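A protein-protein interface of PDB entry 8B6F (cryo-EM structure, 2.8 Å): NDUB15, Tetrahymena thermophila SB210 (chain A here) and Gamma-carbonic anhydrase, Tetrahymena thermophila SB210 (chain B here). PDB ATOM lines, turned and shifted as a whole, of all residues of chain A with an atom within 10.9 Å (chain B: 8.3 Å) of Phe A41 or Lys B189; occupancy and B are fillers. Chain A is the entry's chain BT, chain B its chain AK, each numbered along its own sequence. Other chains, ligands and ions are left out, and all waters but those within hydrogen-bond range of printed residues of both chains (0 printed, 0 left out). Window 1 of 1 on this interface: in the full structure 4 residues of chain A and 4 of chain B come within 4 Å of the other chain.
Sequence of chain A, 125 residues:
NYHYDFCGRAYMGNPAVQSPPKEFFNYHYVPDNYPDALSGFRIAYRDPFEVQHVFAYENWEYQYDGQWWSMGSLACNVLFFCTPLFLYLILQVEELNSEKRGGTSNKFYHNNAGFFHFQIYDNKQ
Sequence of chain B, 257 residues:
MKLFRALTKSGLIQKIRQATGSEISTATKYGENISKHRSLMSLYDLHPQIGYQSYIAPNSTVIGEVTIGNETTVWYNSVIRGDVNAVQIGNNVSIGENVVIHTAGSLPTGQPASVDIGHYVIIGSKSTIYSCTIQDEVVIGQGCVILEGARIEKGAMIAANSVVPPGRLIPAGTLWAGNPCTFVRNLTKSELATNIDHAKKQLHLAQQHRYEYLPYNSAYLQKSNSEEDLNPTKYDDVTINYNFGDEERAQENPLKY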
ATOM      1  N   ASN A  26     -10.338  35.921 -21.683  1.00  0.00           N
ATOM      2  CA  ASN A  26     -11.499  35.077 -21.915  1.00  0.00           C
ATOM      3  C   ASN A  26     -12.026  34.541 -20.592  1.00  0.00           C
ATOM      4  O   ASN A  26     -11.347  34.585 -19.564  1.00  0.00           O
ATOM      5  CB  ASN A  26     -11.161  33.906 -22.846  1.00  0.00           C
ATOM      6  CG  ASN A  26     -12.047  33.860 -24.071  1.00  0.00           C
ATOM      7  OD1 ASN A  26     -11.572  34.000 -25.196  1.00  0.00           O
ATOM      8  ND2 ASN A  26     -13.341  33.655 -23.860  1.00  0.00           N
ATOM      9  N   TYR A  27     -13.261  34.046 -20.630  1.00  0.00           N
ATOM     10  CA  TYR A  27     -13.827  33.372 -19.472  1.00  0.00           C
ATOM     11  C   TYR A  27     -12.989  32.154 -19.108  1.00  0.00           C
ATOM     12  O   TYR A  27     -12.591  31.371 -19.973  1.00  0.00           O
ATOM     13  CB  TYR A  27     -15.265  32.937 -19.755  1.00  0.00           C
ATOM     14  CG  TYR A  27     -16.246  34.075 -19.902  1.00  0.00           C
ATOM     15  CD1 TYR A  27     -16.376  34.756 -21.103  1.00  0.00           C
ATOM     16  CD2 TYR A  27     -17.056  34.454 -18.841  1.00  0.00           C
ATOM     17  CE1 TYR A  27     -17.280  35.791 -21.241  1.00  0.00           C
ATOM     18  CE2 TYR A  27     -17.960  35.486 -18.969  1.00  0.00           C
ATOM     19  CZ  TYR A  27     -18.068  36.150 -20.171  1.00  0.00           C
ATOM     20  OH  TYR A  27     -18.971  37.179 -20.300  1.00  0.00           O
ATOM     21  N   HIS A  28     -12.720  31.998 -17.815  1.00  0.00           N
ATOM     22  CA  HIS A  28     -12.024  30.833 -17.292  1.00  0.00           C
ATOM     23  C   HIS A  28     -12.778  30.306 -16.082  1.00  0.00           C
ATOM     24  O   HIS A  28     -13.376  31.072 -15.321  1.00  0.00           O
ATOM     25  CB  HIS A  28     -10.578  31.160 -16.912  1.00  0.00           C
ATOM     26  CG  HIS A  28      -9.716  31.526 -18.079  1.00  0.00           C
ATOM     27  ND1 HIS A  28      -9.479  30.664 -19.129  1.00  0.00           N
ATOM     28  CD2 HIS A  28      -9.032  32.657 -18.362  1.00  0.00           C
ATOM     29  CE1 HIS A  28      -8.688  31.250 -20.007  1.00  0.00           C
ATOM     30  NE2 HIS A  28      -8.401  32.461 -19.567  1.00  0.00           N
ATOM     31  N   TYR A  29     -12.744  28.988 -15.911  1.00  0.00           N
ATOM     32  CA  TYR A  29     -13.516  28.311 -14.883  1.00  0.00           C
ATOM     33  C   TYR A  29     -12.594  27.561 -13.933  1.00  0.00           C
ATOM     34  O   TYR A  29     -11.492  27.147 -14.301  1.00  0.00           O
ATOM     35  CB  TYR A  29     -14.529  27.344 -15.504  1.00  0.00           C
ATOM     36  CG  TYR A  29     -15.596  28.040 -16.315  1.00  0.00           C
ATOM     37  CD1 TYR A  29     -15.384  28.361 -17.650  1.00  0.00           C
ATOM     38  CD2 TYR A  29     -16.812  28.387 -15.743  1.00  0.00           C
ATOM     39  CE1 TYR A  29     -16.356  29.004 -18.393  1.00  0.00           C
ATOM     40  CE2 TYR A  29     -17.789  29.029 -16.477  1.00  0.00           C
ATOM     41  CZ  TYR A  29     -17.555  29.334 -17.801  1.00  0.00           C
ATOM     42  OH  TYR A  29     -18.525  29.975 -18.537  1.00  0.00           O
ATOM     43  N   ASN A  33     -14.947  22.124 -12.494  1.00  0.00           N
ATOM     44  CA  ASN A  33     -16.174  22.877 -12.286  1.00  0.00           C
ATOM     45  C   ASN A  33     -17.359  22.109 -12.854  1.00  0.00           C
ATOM     46  O   ASN A  33     -17.248  21.445 -13.888  1.00  0.00           O
ATOM     47  CB  ASN A  33     -16.077  24.251 -12.945  1.00  0.00           C
ATOM     48  CG  ASN A  33     -17.373  25.032 -12.858  1.00  0.00           C
ATOM     49  OD1 ASN A  33     -18.155  24.854 -11.925  1.00  0.00           O
ATOM     50  ND2 ASN A  33     -17.608  25.898 -13.834  1.00  0.00           N
ATOM     51  N   TYR A  34     -18.493  22.200 -12.174  1.00  0.00           N
ATOM     52  CA  TYR A  34     -19.712  21.574 -12.667  1.00  0.00           C
ATOM     53  C   TYR A  34     -20.350  22.473 -13.719  1.00  0.00           C
ATOM     54  O   TYR A  34     -20.707  23.614 -13.408  1.00  0.00           O
ATOM     55  CB  TYR A  34     -20.681  21.325 -11.520  1.00  0.00           C
ATOM     56  CG  TYR A  34     -21.937  20.588 -11.918  1.00  0.00           C
ATOM     57  CD1 TYR A  34     -21.871  19.374 -12.588  1.00  0.00           C
ATOM     58  CD2 TYR A  34     -23.189  21.094 -11.601  1.00  0.00           C
ATOM     59  CE1 TYR A  34     -23.017  18.692 -12.945  1.00  0.00           C
ATOM     60  CE2 TYR A  34     -24.341  20.418 -11.953  1.00  0.00           C
ATOM     61  CZ  TYR A  34     -24.248  19.219 -12.625  1.00  0.00           C
ATOM     62  OH  TYR A  34     -25.390  18.542 -12.978  1.00  0.00           O
ATOM     63  N   PRO A  35     -20.509  22.014 -14.962  1.00  0.00           N
ATOM     64  CA  PRO A  35     -21.058  22.891 -16.002  1.00  0.00           C
ATOM     65  C   PRO A  35     -22.482  23.323 -15.694  1.00  0.00           C
ATOM     66  O   PRO A  35     -23.252  22.607 -15.051  1.00  0.00           O
ATOM     67  CB  PRO A  35     -21.003  22.026 -17.268  1.00  0.00           C
ATOM     68  CG  PRO A  35     -20.020  20.964 -16.975  1.00  0.00           C
ATOM     69  CD  PRO A  35     -20.122  20.703 -15.509  1.00  0.00           C
ATOM     70  N   ASP A  36     -22.824  24.517 -16.168  1.00  0.00           N
ATOM     71  CA  ASP A  36     -24.177  25.042 -16.062  1.00  0.00           C
ATOM     72  C   ASP A  36     -24.956  24.584 -17.290  1.00  0.00           C
ATOM     73  O   ASP A  36     -24.573  24.896 -18.422  1.00  0.00           O
ATOM     74  CB  ASP A  36     -24.155  26.565 -15.961  1.00  0.00           C
ATOM     75  CG  ASP A  36     -25.513  27.147 -15.642  1.00  0.00           C
ATOM     76  OD1 ASP A  36     -25.996  26.946 -14.509  1.00  0.00           O
ATOM     77  OD2 ASP A  36     -26.097  27.809 -16.525  1.00  0.00           O
ATOM     78  N   ALA A  37     -26.045  23.854 -17.068  1.00  0.00           N
ATOM     79  CA  ALA A  37     -26.766  23.159 -18.129  1.00  0.00           C
ATOM     80  C   ALA A  37     -28.236  23.543 -18.134  1.00  0.00           C
ATOM     81  O   ALA A  37     -29.124  22.692 -18.224  1.00  0.00           O
ATOM     82  CB  ALA A  37     -26.613  21.649 -17.977  1.00  0.00           C
ATOM     83  N   LEU A  38     -28.521  24.837 -18.039  1.00  0.00           N
ATOM     84  CA  LEU A  38     -29.900  25.295 -18.082  1.00  0.00           C
ATOM     85  C   LEU A  38     -30.362  25.461 -19.521  1.00  0.00           C
ATOM     86  O   LEU A  38     -29.626  25.961 -20.374  1.00  0.00           O
ATOM     87  CB  LEU A  38     -30.047  26.623 -17.340  1.00  0.00           C
ATOM     88  CG  LEU A  38     -31.484  27.116 -17.139  1.00  0.00           C
ATOM     89  CD1 LEU A  38     -32.237  26.221 -16.171  1.00  0.00           C
ATOM     90  CD2 LEU A  38     -31.498  28.557 -16.662  1.00  0.00           C
ATOM     91  N   SER A  39     -31.595  25.033 -19.783  1.00  0.00           N
ATOM     92  CA  SER A  39     -32.229  25.192 -21.089  1.00  0.00           C
ATOM     93  C   SER A  39     -31.489  24.412 -22.176  1.00  0.00           C
ATOM     94  O   SER A  39     -31.199  24.929 -23.257  1.00  0.00           O
ATOM     95  CB  SER A  39     -32.343  26.668 -21.460  1.00  0.00           C
ATOM     96  OG  SER A  39     -33.033  26.805 -22.685  1.00  0.00           O
ATOM     97  N   GLY A  40     -31.185  23.152 -21.884  1.00  0.00           N
ATOM     98  CA  GLY A  40     -30.627  22.251 -22.870  1.00  0.00           C
ATOM     99  C   GLY A  40     -29.119  22.250 -22.986  1.00  0.00           C
ATOM    100  O   GLY A  40     -28.581  21.475 -23.786  1.00  0.00           O
ATOM    101  N   PHE A  41     -28.417  23.086 -22.224  1.00  0.00           N
ATOM    102  CA  PHE A  41     -26.956  23.129 -22.250  1.00  0.00           C
ATOM    103  C   PHE A  41     -26.449  23.420 -23.665  1.00  0.00           C
ATOM    104  O   PHE A  41     -25.680  22.655 -24.251  1.00  0.00           O
ATOM    105  CB  PHE A  41     -26.374  21.816 -21.712  1.00  0.00           C
ATOM    106  CG  PHE A  41     -24.932  21.909 -21.273  1.00  0.00           C
ATOM    107  CD1 PHE A  41     -24.127  22.973 -21.652  1.00  0.00           C
ATOM    108  CD2 PHE A  41     -24.383  20.916 -20.481  1.00  0.00           C
ATOM    109  CE1 PHE A  41     -22.810  23.043 -21.245  1.00  0.00           C
ATOM    110  CE2 PHE A  41     -23.067  20.982 -20.073  1.00  0.00           C
ATOM    111  CZ  PHE A  41     -22.280  22.046 -20.456  1.00  0.00           C
ATOM    112  N   ARG A  42     -26.899  24.547 -24.209  1.00  0.00           N
ATOM    113  CA  ARG A  42     -26.492  25.003 -25.533  1.00  0.00           C
ATOM    114  C   ARG A  42     -25.634  26.250 -25.373  1.00  0.00           C
ATOM    115  O   ARG A  42     -26.101  27.263 -24.845  1.00  0.00           O
ATOM    116  CB  ARG A  42     -27.712  25.293 -26.405  1.00  0.00           C
ATOM    117  CG  ARG A  42     -28.573  24.074 -26.688  1.00  0.00           C
ATOM    118  CD  ARG A  42     -29.880  24.477 -27.346  1.00  0.00           C
ATOM    119  NE  ARG A  42     -30.726  25.241 -26.437  1.00  0.00           N
ATOM    120  CZ  ARG A  42     -31.792  25.936 -26.808  1.00  0.00           C
ATOM    121  NH1 ARG A  42     -32.165  26.006 -28.075  1.00  0.00           N
ATOM    122  NH2 ARG A  42     -32.500  26.581 -25.887  1.00  0.00           N
ATOM    123  N   ILE A  43     -24.391  26.175 -25.840  1.00  0.00           N
ATOM    124  CA  ILE A  43     -23.414  27.247 -25.692  1.00  0.00           C
ATOM    125  C   ILE A  43     -23.026  27.726 -27.082  1.00  0.00           C
ATOM    126  O   ILE A  43     -22.677  26.915 -27.947  1.00  0.00           O
ATOM    127  CB  ILE A  43     -22.170  26.786 -24.913  1.00  0.00           C
ATOM    128  CG1 ILE A  43     -22.569  25.986 -23.668  1.00  0.00           C
ATOM    129  CG2 ILE A  43     -21.313  27.985 -24.532  1.00  0.00           C
ATOM    130  CD1 ILE A  43     -23.316  26.777 -22.628  1.00  0.00           C
ATOM    131  N   ALA A  44     -23.086  29.035 -27.296  1.00  0.00           N
ATOM    132  CA  ALA A  44     -22.698  29.632 -28.564  1.00  0.00           C
ATOM    133  C   ALA A  44     -21.270  30.153 -28.488  1.00  0.00           C
ATOM    134  O   ALA A  44     -20.762  30.478 -27.412  1.00  0.00           O
ATOM    135  CB  ALA A  44     -23.642  30.774 -28.939  1.00  0.00           C
ATOM    136  N   TYR A  45     -20.626  30.230 -29.648  1.00  0.00           N
ATOM    137  CA  TYR A  45     -19.273  30.762 -29.717  1.00  0.00           C
ATOM    138  C   TYR A  45     -19.282  32.267 -29.478  1.00  0.00           C
ATOM    139  O   TYR A  45     -20.060  33.002 -30.093  1.00  0.00           O
ATOM    140  CB  TYR A  45     -18.650  30.443 -31.074  1.00  0.00           C
ATOM    141  CG  TYR A  45     -17.149  30.603 -31.099  1.00  0.00           C
ATOM    142  CD1 TYR A  45     -16.321  29.674 -30.481  1.00  0.00           C
ATOM    143  CD2 TYR A  45     -16.558  31.680 -31.747  1.00  0.00           C
ATOM    144  CE1 TYR A  45     -14.946  29.817 -30.502  1.00  0.00           C
ATOM    145  CE2 TYR A  45     -15.183  31.833 -31.773  1.00  0.00           C
ATOM    146  CZ  TYR A  45     -14.384  30.896 -31.149  1.00  0.00           C
ATOM    147  OH  TYR A  45     -13.016  31.040 -31.174  1.00  0.00           O
ATOM    148  N   ARG A  46     -18.408  32.724 -28.587  1.00  0.00           N
ATOM    149  CA  ARG A  46     -18.419  34.109 -28.145  1.00  0.00           C
ATOM    150  C   ARG A  46     -17.726  34.999 -29.170  1.00  0.00           C
ATOM    151  O   ARG A  46     -16.755  34.598 -29.817  1.00  0.00           O
ATOM    152  CB  ARG A  46     -17.738  34.244 -26.784  1.00  0.00           C
ATOM    153  CG  ARG A  46     -18.341  33.354 -25.709  1.00  0.00           C
ATOM    154  CD  ARG A  46     -17.763  33.662 -24.341  1.00  0.00           C
ATOM    155  NE  ARG A  46     -18.346  32.819 -23.303  1.00  0.00           N
ATOM    156  CZ  ARG A  46     -19.526  33.029 -22.738  1.00  0.00           C
ATOM    157  NH1 ARG A  46     -20.294  34.045 -23.096  1.00  0.00           N
ATOM    158  NH2 ARG A  46     -19.949  32.197 -21.791  1.00  0.00           N
ATOM    159  N   ASP A  47     -18.236  36.215 -29.315  1.00  0.00           N
ATOM    160  CA  ASP A  47     -17.634  37.170 -30.239  1.00  0.00           C
ATOM    161  C   ASP A  47     -16.345  37.727 -29.642  1.00  0.00           C
ATOM    162  O   ASP A  47     -16.343  38.158 -28.486  1.00  0.00           O
ATOM    163  CB  ASP A  47     -18.604  38.306 -30.537  1.00  0.00           C
ATOM    164  CG  ASP A  47     -18.036  39.316 -31.513  1.00  0.00           C
ATOM    165  OD1 ASP A  47     -17.946  38.998 -32.717  1.00  0.00           O
ATOM    166  OD2 ASP A  47     -17.677  40.428 -31.077  1.00  0.00           O
ATOM    167  N   GLY B 173     -11.364  17.201 -28.839  1.00  0.00           N
ATOM    168  CA  GLY B 173     -12.790  17.449 -28.987  1.00  0.00           C
ATOM    169  C   GLY B 173     -13.351  17.063 -30.337  1.00  0.00           C
ATOM    170  O   GLY B 173     -14.175  17.796 -30.896  1.00  0.00           O
ATOM    171  N   ASN B 186     -17.293  17.513 -34.815  1.00  0.00           N
ATOM    172  CA  ASN B 186     -16.799  18.045 -33.558  1.00  0.00           C
ATOM    173  C   ASN B 186     -17.747  17.688 -32.415  1.00  0.00           C
ATOM    174  O   ASN B 186     -18.934  17.421 -32.616  1.00  0.00           O
ATOM    175  CB  ASN B 186     -16.635  19.563 -33.637  1.00  0.00           C
ATOM    176  CG  ASN B 186     -15.596  19.981 -34.649  1.00  0.00           C
ATOM    177  OD1 ASN B 186     -14.637  19.257 -34.907  1.00  0.00           O
ATOM    178  ND2 ASN B 186     -15.780  21.158 -35.233  1.00  0.00           N
ATOM    179  N   LEU B 187     -17.203  17.692 -31.204  1.00  0.00           N
ATOM    180  CA  LEU B 187     -17.960  17.389 -29.999  1.00  0.00           C
ATOM    181  C   LEU B 187     -18.256  18.679 -29.247  1.00  0.00           C
ATOM    182  O   LEU B 187     -17.409  19.574 -29.172  1.00  0.00           O
ATOM    183  CB  LEU B 187     -17.193  16.415 -29.102  1.00  0.00           C
ATOM    184  CG  LEU B 187     -16.971  15.018 -29.684  1.00  0.00           C
ATOM    185  CD1 LEU B 187     -16.041  14.221 -28.798  1.00  0.00           C
ATOM    186  CD2 LEU B 187     -18.287  14.281 -29.862  1.00  0.00           C
ATOM    187  N   THR B 188     -19.459  18.767 -28.691  1.00  0.00           N
ATOM    188  CA  THR B 188     -19.912  19.969 -28.009  1.00  0.00           C
ATOM    189  C   THR B 188     -19.612  19.892 -26.515  1.00  0.00           C
ATOM    190  O   THR B 188     -19.312  18.832 -25.965  1.00  0.00           O
ATOM    191  CB  THR B 188     -21.410  20.178 -28.231  1.00  0.00           C
ATOM    192  OG1 THR B 188     -22.133  19.036 -27.756  1.00  0.00           O
ATOM    193  CG2 THR B 188     -21.707  20.383 -29.706  1.00  0.00           C
ATOM    194  N   LYS B 189     -19.704  21.048 -25.855  1.00  0.00           N
ATOM    195  CA  LYS B 189     -19.459  21.101 -24.417  1.00  0.00           C
ATOM    196  C   LYS B 189     -20.385  20.163 -23.658  1.00  0.00           C
ATOM    197  O   LYS B 189     -19.993  19.603 -22.628  1.00  0.00           O
ATOM    198  CB  LYS B 189     -19.621  22.532 -23.910  1.00  0.00           C
ATOM    199  CG  LYS B 189     -18.662  23.522 -24.546  1.00  0.00           C
ATOM    200  CD  LYS B 189     -18.735  24.873 -23.856  1.00  0.00           C
ATOM    201  CE  LYS B 189     -17.800  25.881 -24.502  1.00  0.00           C
ATOM    202  NZ  LYS B 189     -18.192  26.184 -25.907  1.00  0.00           N
ATOM    203  N   SER B 190     -21.614  19.982 -24.142  1.00  0.00           N
ATOM    204  CA  SER B 190     -22.525  19.044 -23.500  1.00  0.00           C
ATOM    205  C   SER B 190     -21.986  17.620 -23.574  1.00  0.00           C
ATOM    206  O   SER B 190     -22.042  16.876 -22.588  1.00  0.00           O
ATOM    207  CB  SER B 190     -23.908  19.131 -24.141  1.00  0.00           C
ATOM    208  OG  SER B 190     -23.840  18.885 -25.533  1.00  0.00           O
ATOM    209  N   GLU B 191     -21.466  17.219 -24.736  1.00  0.00           N
ATOM    210  CA  GLU B 191     -20.894  15.881 -24.857  1.00  0.00           C
ATOM    211  C   GLU B 191     -19.683  15.719 -23.950  1.00  0.00           C
ATOM    212  O   GLU B 191     -19.520  14.682 -23.298  1.00  0.00           O
ATOM    213  CB  GLU B 191     -20.511  15.604 -26.311  1.00  0.00           C
ATOM    214  CG  GLU B 191     -21.658  15.743 -27.296  1.00  0.00           C
ATOM    215  CD  GLU B 191     -22.745  14.707 -27.079  1.00  0.00           C
ATOM    216  OE1 GLU B 191     -22.550  13.800 -26.242  1.00  0.00           O
ATOM    217  OE2 GLU B 191     -23.795  14.796 -27.750  1.00  0.00           O
ATOM    218  N   LEU B 192     -18.816  16.731 -23.899  1.00  0.00           N
ATOM    219  CA  LEU B 192     -17.647  16.659 -23.030  1.00  0.00           C
ATOM    220  C   LEU B 192     -18.061  16.549 -21.569  1.00  0.00           C
ATOM    221  O   LEU B 192     -17.479  15.769 -20.805  1.00  0.00           O
ATOM    222  CB  LEU B 192     -16.752  17.877 -23.248  1.00  0.00           C
ATOM    223  CG  LEU B 192     -16.299  18.123 -24.689  1.00  0.00           C
ATOM    224  CD1 LEU B 192     -15.458  19.381 -24.771  1.00  0.00           C
ATOM    225  CD2 LEU B 192     -15.529  16.931 -25.234  1.00  0.00           C
ATOM    226  N   ALA B 193     -19.061  17.329 -21.160  1.00  0.00           N
ATOM    227  CA  ALA B 193     -19.549  17.255 -19.788  1.00  0.00           C
ATOM    228  C   ALA B 193     -20.133  15.882 -19.485  1.00  0.00           C
ATOM    229  O   ALA B 193     -19.948  15.348 -18.386  1.00  0.00           O
ATOM    230  CB  ALA B 193     -20.590  18.343 -19.543  1.00  0.00           C
ATOM    231  N   THR B 194     -20.851  15.299 -20.445  1.00  0.00           N
ATOM    232  CA  THR B 194     -21.402  13.964 -20.239  1.00  0.00           C
ATOM    233  C   THR B 194     -20.295  12.938 -20.040  1.00  0.00           C
ATOM    234  O   THR B 194     -20.393  12.073 -19.162  1.00  0.00           O
ATOM    235  CB  THR B 194     -22.279  13.570 -21.427  1.00  0.00           C
ATOM    236  OG1 THR B 194     -23.269  14.581 -21.653  1.00  0.00           O
ATOM    237  CG2 THR B 194     -22.973  12.246 -21.162  1.00  0.00           C
ATOM    238  N   ASN B 195     -19.234  13.012 -20.845  1.00  0.00           N
ATOM    239  CA  ASN B 195     -18.125  12.077 -20.690  1.00  0.00           C
ATOM    240  C   ASN B 195     -17.468  12.232 -19.325  1.00  0.00           C
ATOM    241  O   ASN B 195     -17.188  11.242 -18.641  1.00  0.00           O
ATOM    242  CB  ASN B 195     -17.102  12.290 -21.804  1.00  0.00           C
ATOM    243  CG  ASN B 195     -17.700  12.113 -23.183  1.00  0.00           C
ATOM    244  OD1 ASN B 195     -18.704  11.423 -23.351  1.00  0.00           O
ATOM    245  ND2 ASN B 195     -17.084  12.736 -24.178  1.00  0.00           N
ATOM    246  N   ILE B 196     -17.223  13.473 -18.906  1.00  0.00           N
ATOM    247  CA  ILE B 196     -16.623  13.710 -17.595  1.00  0.00           C
ATOM    248  C   ILE B 196     -17.529  13.171 -16.499  1.00  0.00           C
ATOM    249  O   ILE B 196     -17.062  12.593 -15.511  1.00  0.00           O
ATOM    250  CB  ILE B 196     -16.332  15.209 -17.402  1.00  0.00           C
ATOM    251  CG1 ILE B 196     -15.310  15.689 -18.432  1.00  0.00           C
ATOM    252  CG2 ILE B 196     -15.819  15.477 -15.993  1.00  0.00           C
ATOM    253  CD1 ILE B 196     -15.144  17.196 -18.474  1.00  0.00           C
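The side-chain hydroxyl of Thr B188 sits at hydrogen-bond distance from the side-chain hydroxyl of Ser B190. OG1 of Thr B194 is in hydrogen-bond range of O of Ser B190, at 2.8 Å.
Pro A35 touches Ala B193. CZ of Phe A41 touches O of Lys B189, 3.99 Å away. Ser B190 touches Phe A41. CE2 of Phe A41 touches CB of Ala B193, at 3.7 Å. NZ of Lys B189 touches CG2 of Ile A43, at 3.9 Å.
Tyr A27 touches none of the printed residues of chain B. Printed residues of chain B within 4 Å of Pro A35: Ala B193 (3.7 Å). No residue of chain B comes within 4 Å of Gly A40. Of the printed residues of chain B, Ile A43 touches Lys B189. No residue of chain A comes within 4 Å of Thr B188. Printed residues of chain A within 4 Å of Lys B189: Phe A41 (3.99 Å) and Ile A43 (3.9 Å). No residue of chain A comes within 4 Å of Leu B192. Of chain A, only Pro A35 (3.7 Å) and Phe A41 (3.7 Å) come within 4 Å of Ala B193. The nearest printed residue of chain A that does not touch Lys B189 is Ala A44 (5.2 Å).
Hydrophobic or aromatic side chains of chain B within 4 Å of the printed part of chain A: Ala B193. Hydrophobic or aromatic side chains of chain A that line the printed part of chain B: Pro A35, Phe A41 and Ile A43. Among the printed residues, 5 pairs touch across the chains. Among the printed residues, no Asp or Glu carboxylate lies within 4 Å of a Lys or Arg side-chain nitrogen of the other chain.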
